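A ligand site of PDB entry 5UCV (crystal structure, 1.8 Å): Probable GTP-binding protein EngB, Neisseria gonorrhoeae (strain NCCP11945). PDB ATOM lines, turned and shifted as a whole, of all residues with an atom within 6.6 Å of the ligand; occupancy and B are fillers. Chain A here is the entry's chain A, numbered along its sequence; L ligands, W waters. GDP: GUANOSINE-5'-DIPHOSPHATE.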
ATOM      1  N   GLY A  38     -20.054  10.102  14.753  1.00  0.00           N
ATOM      2  CA  GLY A  38     -19.997   9.683  13.370  1.00  0.00           C
ATOM      3  C   GLY A  38     -18.815  10.301  12.671  1.00  0.00           C
ATOM      4  O   GLY A  38     -18.184  11.240  13.170  1.00  0.00           O
ATOM      5  N   ARG A  39     -18.514   9.754  11.500  1.00  0.00           N
ATOM      6  CA  ARG A  39     -17.443  10.296  10.676  1.00  0.00           C
ATOM      7  C   ARG A  39     -17.839  11.688  10.183  1.00  0.00           C
ATOM      8  O   ARG A  39     -19.020  12.004   9.994  1.00  0.00           O
ATOM      9  CB  ARG A  39     -17.164   9.362   9.491  1.00  0.00           C
ATOM     10  CG  ARG A  39     -15.895   9.642   8.687  1.00  0.00           C
ATOM     11  CD  ARG A  39     -15.658   8.528   7.646  1.00  0.00           C
ATOM     12  NE  ARG A  39     -14.503   8.755   6.779  1.00  0.00           N
ATOM     13  CZ  ARG A  39     -13.254   8.387   7.057  1.00  0.00           C
ATOM     14  NH1 ARG A  39     -12.981   7.765   8.193  1.00  0.00           N
ATOM     15  NH2 ARG A  39     -12.269   8.630   6.194  1.00  0.00           N
ATOM     16  N   SER A  40     -16.834  12.542   9.994  1.00  0.00           N
ATOM     17  CA  SER A  40     -17.096  13.838   9.415  1.00  0.00           C
ATOM     18  C   SER A  40     -17.841  13.664   8.094  1.00  0.00           C
ATOM     19  O   SER A  40     -17.557  12.745   7.323  1.00  0.00           O
ATOM     20  CB  SER A  40     -15.804  14.625   9.209  1.00  0.00           C
ATOM     21  OG  SER A  40     -15.333  15.132  10.446  1.00  0.00           O
ATOM     22  N   ASN A  41     -18.820  14.536   7.857  1.00  0.00           N
ATOM     23  CA  ASN A  41     -19.659  14.524   6.663  1.00  0.00           C
ATOM     24  C   ASN A  41     -20.579  13.311   6.572  1.00  0.00           C
ATOM     25  O   ASN A  41     -21.082  13.000   5.500  1.00  0.00           O
ATOM     26  CB  ASN A  41     -18.805  14.637   5.392  1.00  0.00           C
ATOM     27  CG  ASN A  41     -19.456  15.521   4.345  1.00  0.00           C
ATOM     28  OD1 ASN A  41     -19.507  16.743   4.490  1.00  0.00           O
ATOM     29  ND2 ASN A  41     -19.958  14.909   3.273  1.00  0.00           N
ATOM     30  N   ALA A  42     -20.814  12.606   7.687  1.00  0.00           N
ATOM     31  CA  ALA A  42     -21.828  11.555   7.698  1.00  0.00           C
ATOM     32  C   ALA A  42     -23.245  12.119   7.674  1.00  0.00           C
ATOM     33  O   ALA A  42     -24.174  11.366   7.344  1.00  0.00           O
ATOM     34  CB  ALA A  42     -21.673  10.659   8.937  1.00  0.00           C
ATOM     35  N   GLY A  43     -23.418  13.393   7.983  1.00  0.00           N
ATOM     36  CA  GLY A  43     -24.737  13.978   8.176  1.00  0.00           C
ATOM     37  C   GLY A  43     -25.182  14.086   9.622  1.00  0.00           C
ATOM     38  O   GLY A  43     -26.385  14.159   9.868  1.00  0.00           O
ATOM     39  N   LYS A  44     -24.251  14.132  10.576  1.00  0.00           N
ATOM     40  CA  LYS A  44     -24.650  14.125  11.986  1.00  0.00           C
ATOM     41  C   LYS A  44     -25.296  15.445  12.400  1.00  0.00           C
ATOM     42  O   LYS A  44     -26.291  15.453  13.129  1.00  0.00           O
ATOM     43  CB  LYS A  44     -23.435  13.800  12.860  1.00  0.00           C
ATOM     44  CG  LYS A  44     -23.666  14.011  14.343  1.00  0.00           C
ATOM     45  CD  LYS A  44     -22.623  13.270  15.222  1.00  0.00           C
ATOM     46  CE  LYS A  44     -21.190  13.750  14.968  1.00  0.00           C
ATOM     47  NZ  LYS A  44     -20.981  15.212  15.292  1.00  0.00           N
ATOM     48  N   SER A  45     -24.728  16.572  11.980  1.00  0.00           N
ATOM     49  CA  SER A  45     -25.315  17.863  12.318  1.00  0.00           C
ATOM     50  C   SER A  45     -26.718  17.994  11.732  1.00  0.00           C
ATOM     51  O   SER A  45     -27.648  18.457  12.409  1.00  0.00           O
ATOM     52  CB  SER A  45     -24.413  18.997  11.827  1.00  0.00           C
ATOM     53  OG  SER A  45     -25.075  20.239  11.921  1.00  0.00           O
ATOM     54  N   SER A  46     -26.880  17.587  10.479  1.00  0.00           N
ATOM     55  CA  SER A  46     -28.201  17.632   9.858  1.00  0.00           C
ATOM     56  C   SER A  46     -29.185  16.726  10.595  1.00  0.00           C
ATOM     57  O   SER A  46     -30.339  17.109  10.807  1.00  0.00           O
ATOM     58  CB  SER A  46     -28.091  17.221   8.384  1.00  0.00           C
ATOM     59  OG  SER A  46     -27.300  18.170   7.677  1.00  0.00           O
ATOM     60  N   ALA A  47     -28.743  15.518  10.981  1.00  0.00           N
ATOM     61  CA  ALA A  47     -29.612  14.605  11.703  1.00  0.00           C
ATOM     62  C   ALA A  47     -30.064  15.188  13.039  1.00  0.00           C
ATOM     63  O   ALA A  47     -31.237  15.083  13.399  1.00  0.00           O
ATOM     64  CB  ALA A  47     -28.905  13.263  11.900  1.00  0.00           C
ATOM     65  N   ASN A  49     -30.255  18.399  13.802  1.00  0.00           N
ATOM     66  CA  ASN A  49     -31.184  19.490  13.523  1.00  0.00           C
ATOM     67  C   ASN A  49     -32.561  18.946  13.173  1.00  0.00           C
ATOM     68  O   ASN A  49     -33.586  19.487  13.607  1.00  0.00           O
ATOM     69  CB  ASN A  49     -30.651  20.367  12.390  1.00  0.00           C
ATOM     70  CG  ASN A  49     -29.428  21.151  12.787  1.00  0.00           C
ATOM     71  OD1 ASN A  49     -29.198  21.416  13.975  1.00  0.00           O
ATOM     72  ND2 ASN A  49     -28.622  21.536  11.805  1.00  0.00           N
ATOM     73  N   GLY A  86     -17.102  15.061  14.739  1.00  0.00           N
ATOM     74  CA  GLY A  86     -16.940  13.994  13.773  1.00  0.00           C
ATOM     75  C   GLY A  86     -15.473  13.617  13.608  1.00  0.00           C
ATOM     76  O   GLY A  86     -14.586  14.477  13.635  1.00  0.00           O
ATOM     77  N   ILE A 120     -23.931   7.492  13.574  1.00  0.00           N
ATOM     78  CA  ILE A 120     -24.427   7.958  12.292  1.00  0.00           C
ATOM     79  C   ILE A 120     -23.404   7.602  11.224  1.00  0.00           C
ATOM     80  O   ILE A 120     -22.208   7.885  11.386  1.00  0.00           O
ATOM     81  CB  ILE A 120     -24.691   9.472  12.328  1.00  0.00           C
ATOM     82  CG1 ILE A 120     -25.719   9.781  13.418  1.00  0.00           C
ATOM     83  CG2 ILE A 120     -25.134   9.969  10.961  1.00  0.00           C
ATOM     84  CD1 ILE A 120     -26.150  11.210  13.476  1.00  0.00           C
ATOM     85  N   ARG A 124     -24.131   5.492   1.956  1.00  0.00           N
ATOM     86  CA  ARG A 124     -23.384   5.131   0.765  1.00  0.00           C
ATOM     87  C   ARG A 124     -22.062   4.440   1.102  1.00  0.00           C
ATOM     88  O   ARG A 124     -21.594   3.611   0.318  1.00  0.00           O
ATOM     89  CB  ARG A 124     -23.127   6.371  -0.081  1.00  0.00           C
ATOM     90  CG  ARG A 124     -24.383   7.045  -0.637  1.00  0.00           C
ATOM     91  CD  ARG A 124     -24.062   8.429  -1.212  1.00  0.00           C
ATOM     92  NE  ARG A 124     -23.471   9.305  -0.197  1.00  0.00           N
ATOM     93  CZ  ARG A 124     -22.800  10.421  -0.460  1.00  0.00           C
ATOM     94  NH1 ARG A 124     -22.603  10.805  -1.723  1.00  0.00           N
ATOM     95  NH2 ARG A 124     -22.298  11.144   0.534  1.00  0.00           N
ATOM     96  N   SER A 150     -27.487   7.303   7.318  1.00  0.00           N
ATOM     97  CA  SER A 150     -27.939   8.623   6.919  1.00  0.00           C
ATOM     98  C   SER A 150     -27.795   8.856   5.418  1.00  0.00           C
ATOM     99  O   SER A 150     -27.138   8.094   4.701  1.00  0.00           O
ATOM    100  CB  SER A 150     -27.144   9.683   7.669  1.00  0.00           C
ATOM    101  OG  SER A 150     -25.753   9.484   7.436  1.00  0.00           O
ATOM    102  N   LYS A 151     -28.405   9.953   4.954  1.00  0.00           N
ATOM    103  CA  LYS A 151     -28.450  10.290   3.528  1.00  0.00           C
ATOM    104  C   LYS A 151     -29.046   9.153   2.713  1.00  0.00           C
ATOM    105  O   LYS A 151     -28.658   8.930   1.562  1.00  0.00           O
ATOM    106  CB  LYS A 151     -27.066  10.643   2.985  1.00  0.00           C
ATOM    107  CG  LYS A 151     -26.256  11.589   3.858  1.00  0.00           C
ATOM    108  CD  LYS A 151     -24.933  11.928   3.188  1.00  0.00           C
ATOM    109  CE  LYS A 151     -24.059  12.787   4.086  1.00  0.00           C
ATOM    110  NZ  LYS A 151     -22.751  13.101   3.414  1.00  0.00           N
ATOM    111  N   ALA A 152     -29.989   8.403   3.300  1.00  0.00           N
ATOM    112  CA  ALA A 152     -30.546   7.253   2.606  1.00  0.00           C
ATOM    113  C   ALA A 152     -31.224   7.661   1.306  1.00  0.00           C
ATOM    114  O   ALA A 152     -31.300   6.860   0.378  1.00  0.00           O
ATOM    115  CB  ALA A 152     -31.544   6.517   3.514  1.00  0.00           C
ATOM    116  N   ASP A 153     -31.693   8.908   1.214  1.00  0.00           N
ATOM    117  CA  ASP A 153     -32.340   9.408   0.002  1.00  0.00           C
ATOM    118  C   ASP A 153     -31.409   9.440  -1.202  1.00  0.00           C
ATOM    119  O   ASP A 153     -31.900   9.575  -2.331  1.00  0.00           O
ATOM    120  CB  ASP A 153     -32.896  10.809   0.245  1.00  0.00           C
ATOM    121  CG  ASP A 153     -31.822  11.784   0.669  1.00  0.00           C
ATOM    122  OD1 ASP A 153     -31.382  11.741   1.837  1.00  0.00           O
ATOM    123  OD2 ASP A 153     -31.380  12.591  -0.176  1.00  0.00           O
ATOM    124  N   LYS A 154     -30.099   9.335  -0.998  1.00  0.00           N
ATOM    125  CA  LYS A 154     -29.140   9.313  -2.099  1.00  0.00           C
ATOM    126  C   LYS A 154     -28.968   7.926  -2.711  1.00  0.00           C
ATOM    127  O   LYS A 154     -28.221   7.788  -3.678  1.00  0.00           O
ATOM    128  CB  LYS A 154     -27.793   9.849  -1.611  1.00  0.00           C
ATOM    129  CG  LYS A 154     -27.876  11.270  -1.064  1.00  0.00           C
ATOM    130  CD  LYS A 154     -26.517  11.813  -0.677  1.00  0.00           C
ATOM    131  CE  LYS A 154     -25.753  12.334  -1.887  1.00  0.00           C
ATOM    132  NZ  LYS A 154     -24.501  13.028  -1.484  1.00  0.00           N
ATOM    133  N   PHE A 185     -32.107   6.433   7.463  1.00  0.00           N
ATOM    134  CA  PHE A 185     -32.448   7.771   7.931  1.00  0.00           C
ATOM    135  C   PHE A 185     -32.197   8.769   6.815  1.00  0.00           C
ATOM    136  O   PHE A 185     -31.219   8.642   6.062  1.00  0.00           O
ATOM    137  CB  PHE A 185     -31.616   8.126   9.181  1.00  0.00           C
ATOM    138  CG  PHE A 185     -32.105   9.356   9.890  1.00  0.00           C
ATOM    139  CD1 PHE A 185     -33.066   9.255  10.893  1.00  0.00           C
ATOM    140  CD2 PHE A 185     -31.599  10.618   9.573  1.00  0.00           C
ATOM    141  CE1 PHE A 185     -33.510  10.396  11.546  1.00  0.00           C
ATOM    142  CE2 PHE A 185     -32.058  11.744  10.221  1.00  0.00           C
ATOM    143  CZ  PHE A 185     -33.008  11.629  11.212  1.00  0.00           C
ATOM    144  N   SER A 186     -33.070   9.768   6.700  1.00  0.00           N
ATOM    145  CA  SER A 186     -32.828  10.883   5.785  1.00  0.00           C
ATOM    146  C   SER A 186     -33.283  12.177   6.449  1.00  0.00           C
ATOM    147  O   SER A 186     -34.491  12.388   6.630  1.00  0.00           O
ATOM    148  CB  SER A 186     -33.541  10.709   4.447  1.00  0.00           C
ATOM    149  OG  SER A 186     -33.380  11.901   3.690  1.00  0.00           O
ATOM    150  N   SER A 187     -32.332  13.040   6.773  1.00  0.00           N
ATOM    151  CA  SER A 187     -32.659  14.378   7.237  1.00  0.00           C
ATOM    152  C   SER A 187     -33.421  15.139   6.171  1.00  0.00           C
ATOM    153  O   SER A 187     -34.412  15.824   6.455  1.00  0.00           O
ATOM    154  CB  SER A 187     -31.396  15.140   7.615  1.00  0.00           C
ATOM    155  OG  SER A 187     -30.745  14.531   8.705  1.00  0.00           O
ATOM    156  N   LEU A 188     -32.964  15.022   4.924  1.00  0.00           N
ATOM    157  CA  LEU A 188     -33.555  15.793   3.836  1.00  0.00           C
ATOM    158  C   LEU A 188     -35.041  15.482   3.668  1.00  0.00           C
ATOM    159  O   LEU A 188     -35.868  16.395   3.591  1.00  0.00           O
ATOM    160  CB  LEU A 188     -32.796  15.521   2.532  1.00  0.00           C
ATOM    161  CG  LEU A 188     -33.196  16.392   1.337  1.00  0.00           C
ATOM    162  CD1 LEU A 188     -32.846  17.849   1.613  1.00  0.00           C
ATOM    163  CD2 LEU A 188     -32.518  15.895   0.073  1.00  0.00           C
ATOM    164  N   LYS A 189     -35.383  14.202   3.632  1.00  0.00           N
ATOM    165  CA  LYS A 189     -36.764  13.777   3.401  1.00  0.00           C
ATOM    166  C   LYS A 189     -37.513  13.496   4.696  1.00  0.00           C
ATOM    167  O   LYS A 189     -38.619  12.943   4.636  1.00  0.00           O
ATOM    168  CB  LYS A 189     -36.773  12.535   2.504  1.00  0.00           C
ATOM    169  CG  LYS A 189     -36.070  12.738   1.168  1.00  0.00           C
ATOM    170  CD  LYS A 189     -36.764  13.837   0.369  1.00  0.00           C
ATOM    171  CE  LYS A 189     -35.990  14.215  -0.879  1.00  0.00           C
ATOM    172  NZ  LYS A 189     -36.667  15.326  -1.624  1.00  0.00           N
HETATM  173  PB  GDP L   1     -21.576  16.263   9.529  1.00  0.00           P
HETATM  174  O1B GDP L   1     -22.163  17.134  10.625  1.00  0.00           O
HETATM  175  O2B GDP L   1     -21.528  14.806   9.946  1.00  0.00           O
HETATM  176  O3B GDP L   1     -20.180  16.745   9.182  1.00  0.00           O
HETATM  177  O3A GDP L   1     -22.489  16.285   8.199  1.00  0.00           O
HETATM  178  PA  GDP L   1     -23.512  17.470   7.780  1.00  0.00           P
HETATM  179  O1A GDP L   1     -24.832  17.421   8.503  1.00  0.00           O
HETATM  180  O2A GDP L   1     -22.842  18.820   7.856  1.00  0.00           O
HETATM  181  O5' GDP L   1     -23.785  17.014   6.240  1.00  0.00           O
HETATM  182  C5' GDP L   1     -22.692  16.870   5.332  1.00  0.00           C
HETATM  183  C4' GDP L   1     -23.204  17.043   3.908  1.00  0.00           C
HETATM  184  O4' GDP L   1     -24.201  16.047   3.653  1.00  0.00           O
HETATM  185  C3' GDP L   1     -23.881  18.390   3.740  1.00  0.00           C
HETATM  186  O3' GDP L   1     -23.549  18.918   2.456  1.00  0.00           O
HETATM  187  C2' GDP L   1     -25.356  18.102   3.773  1.00  0.00           C
HETATM  188  O2' GDP L   1     -26.011  18.989   2.854  1.00  0.00           O
HETATM  189  C1' GDP L   1     -25.442  16.659   3.301  1.00  0.00           C
HETATM  190  N9  GDP L   1     -26.526  15.913   3.961  1.00  0.00           N
HETATM  191  C8  GDP L   1     -26.703  15.742   5.294  1.00  0.00           C
HETATM  192  N7  GDP L   1     -27.806  14.990   5.540  1.00  0.00           N
HETATM  193  C5  GDP L   1     -28.326  14.640   4.339  1.00  0.00           C
HETATM  194  C6  GDP L   1     -29.489  13.843   3.850  1.00  0.00           C
HETATM  195  O6  GDP L   1     -30.270  13.274   4.647  1.00  0.00           O
HETATM  196  N1  GDP L   1     -29.672  13.731   2.528  1.00  0.00           N
HETATM  197  C2  GDP L   1     -28.864  14.322   1.633  1.00  0.00           C
HETATM  198  N2  GDP L   1     -29.126  14.165   0.314  1.00  0.00           N
HETATM  199  N3  GDP L   1     -27.782  15.059   1.997  1.00  0.00           N
HETATM  200  C4  GDP L   1     -27.479  15.241   3.309  1.00  0.00           C
HETATM  201  O   HOH W   1     -19.476  18.257   6.977  1.00  0.00           O
HETATM  202  O   HOH W   2     -21.466  17.069  13.301  1.00  0.00           O
HETATM  203  O   HOH W   3     -22.973  14.612   0.839  1.00  0.00           O
HETATM  204  O   HOH W   4     -28.728  15.990  -1.870  1.00  0.00           O
HETATM  205  O   HOH W   5     -28.160  13.676   8.061  1.00  0.00           O
HETATM  206  O   HOH W   6     -21.426  20.363   5.792  1.00  0.00           O
HETATM  207  O   HOH W   7     -19.946  13.986  11.763  1.00  0.00           O
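An oxygen (O3A) of the ligand is in hydrogen-bond range of the backbone NH of Gly 43 (3.0 Å). The side-chain hydroxyl of Ser 46 is in hydrogen-bond range of an oxygen (O1A) of the ligand, at 2.7 Å. NZ of Lys 151 sits close to O4' of the ligand, at 3.3 Å. N of Ser 45 lies within hydrogen-bond range of O1B of the ligand. The backbone NH of Asn 41 sits at hydrogen-bond distance from an oxygen (O3B) of the ligand (2.9 Å). The backbone NH of Lys 44 lies within hydrogen-bond range of an oxygen (O2B) of the ligand, at 2.9 Å. An oxygen (O1A) of the ligand lies within hydrogen-bond range of the backbone NH (N) of Ser 46. OD1 of Asp 153 sits at hydrogen-bond distance from N1 of the ligand (2.7 Å). The backbone NH (N) of Leu 188 sits at hydrogen-bond distance from an oxygen (O6) of the ligand. The backbone NH (N) of Ser 187 is in hydrogen-bond range of an oxygen (O6) of the ligand (3.0 Å). The backbone NH (N) of Ala 42 sits at hydrogen-bond distance from an oxygen (O2B) of the ligand (3.2 Å).
OD1 of Asp 153 is in hydrogen-bond range of OG of Ser 186. The backbone NH (N) of Leu 188 sits close to the side-chain hydroxyl (OG) of Ser 186 (3.4 Å). The backbone carbonyl oxygen of Ala 42 is in hydrogen-bond range of the side-chain hydroxyl of Ser 150. The side-chain amide nitrogen (ND2) of Asn 49 sits close to the backbone carbonyl oxygen (O) of Ser 45 (3.3 Å). The backbone carbonyl oxygen of Asn 41 is in hydrogen-bond range of the side-chain amino group of Lys 151. N of Lys 189 is in hydrogen-bond range of OG of Ser 186 (3.1 Å). The backbone NH of Lys 151 is in hydrogen-bond range of the backbone carbonyl oxygen of Phe 185, at 3.3 Å. The side-chain hydroxyl (OG) of Ser 187 lies close to the backbone carbonyl oxygen (O) of Ser 46, 3.4 Å away.
Arg 39 touches the ligand. CG of Lys 154 touches N2 of the ligand, at 3.4 Å. OG of Ser 186 touches O6 of the ligand, at 3.5 Å. Within 4 Å of the ligand: Arg 39, Asn 41, Ala 42, Gly 43, Lys 44, Ser 45, Ser 46, Lys 151, Asp 153, Lys 154, Ser 186, Ser 187 and Leu 188. The nearest printed residue that does not touch the ligand is Ser 40 (4.02 Å).
Water W7 lies within hydrogen-bond range of O2B of the ligand and O of Arg 39. Water W1 bridges O3B of the ligand and OD1 of Asn 41. Water W2 lies within hydrogen-bond range of the side-chain amino group (NZ) of Lys 44 and an oxygen (O1B) of the ligand. Water W5 lies within hydrogen-bond range of O of Gly 43 (2.6 Å), OG of Ser 187 (2.8 Å) and N7 of the ligand (2.9 Å). Water W3 lies within hydrogen-bond range of NZ of Lys 151 (3.0 Å), NZ of Lys 154 (3.2 Å) and O4' of the ligand (3.4 Å).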
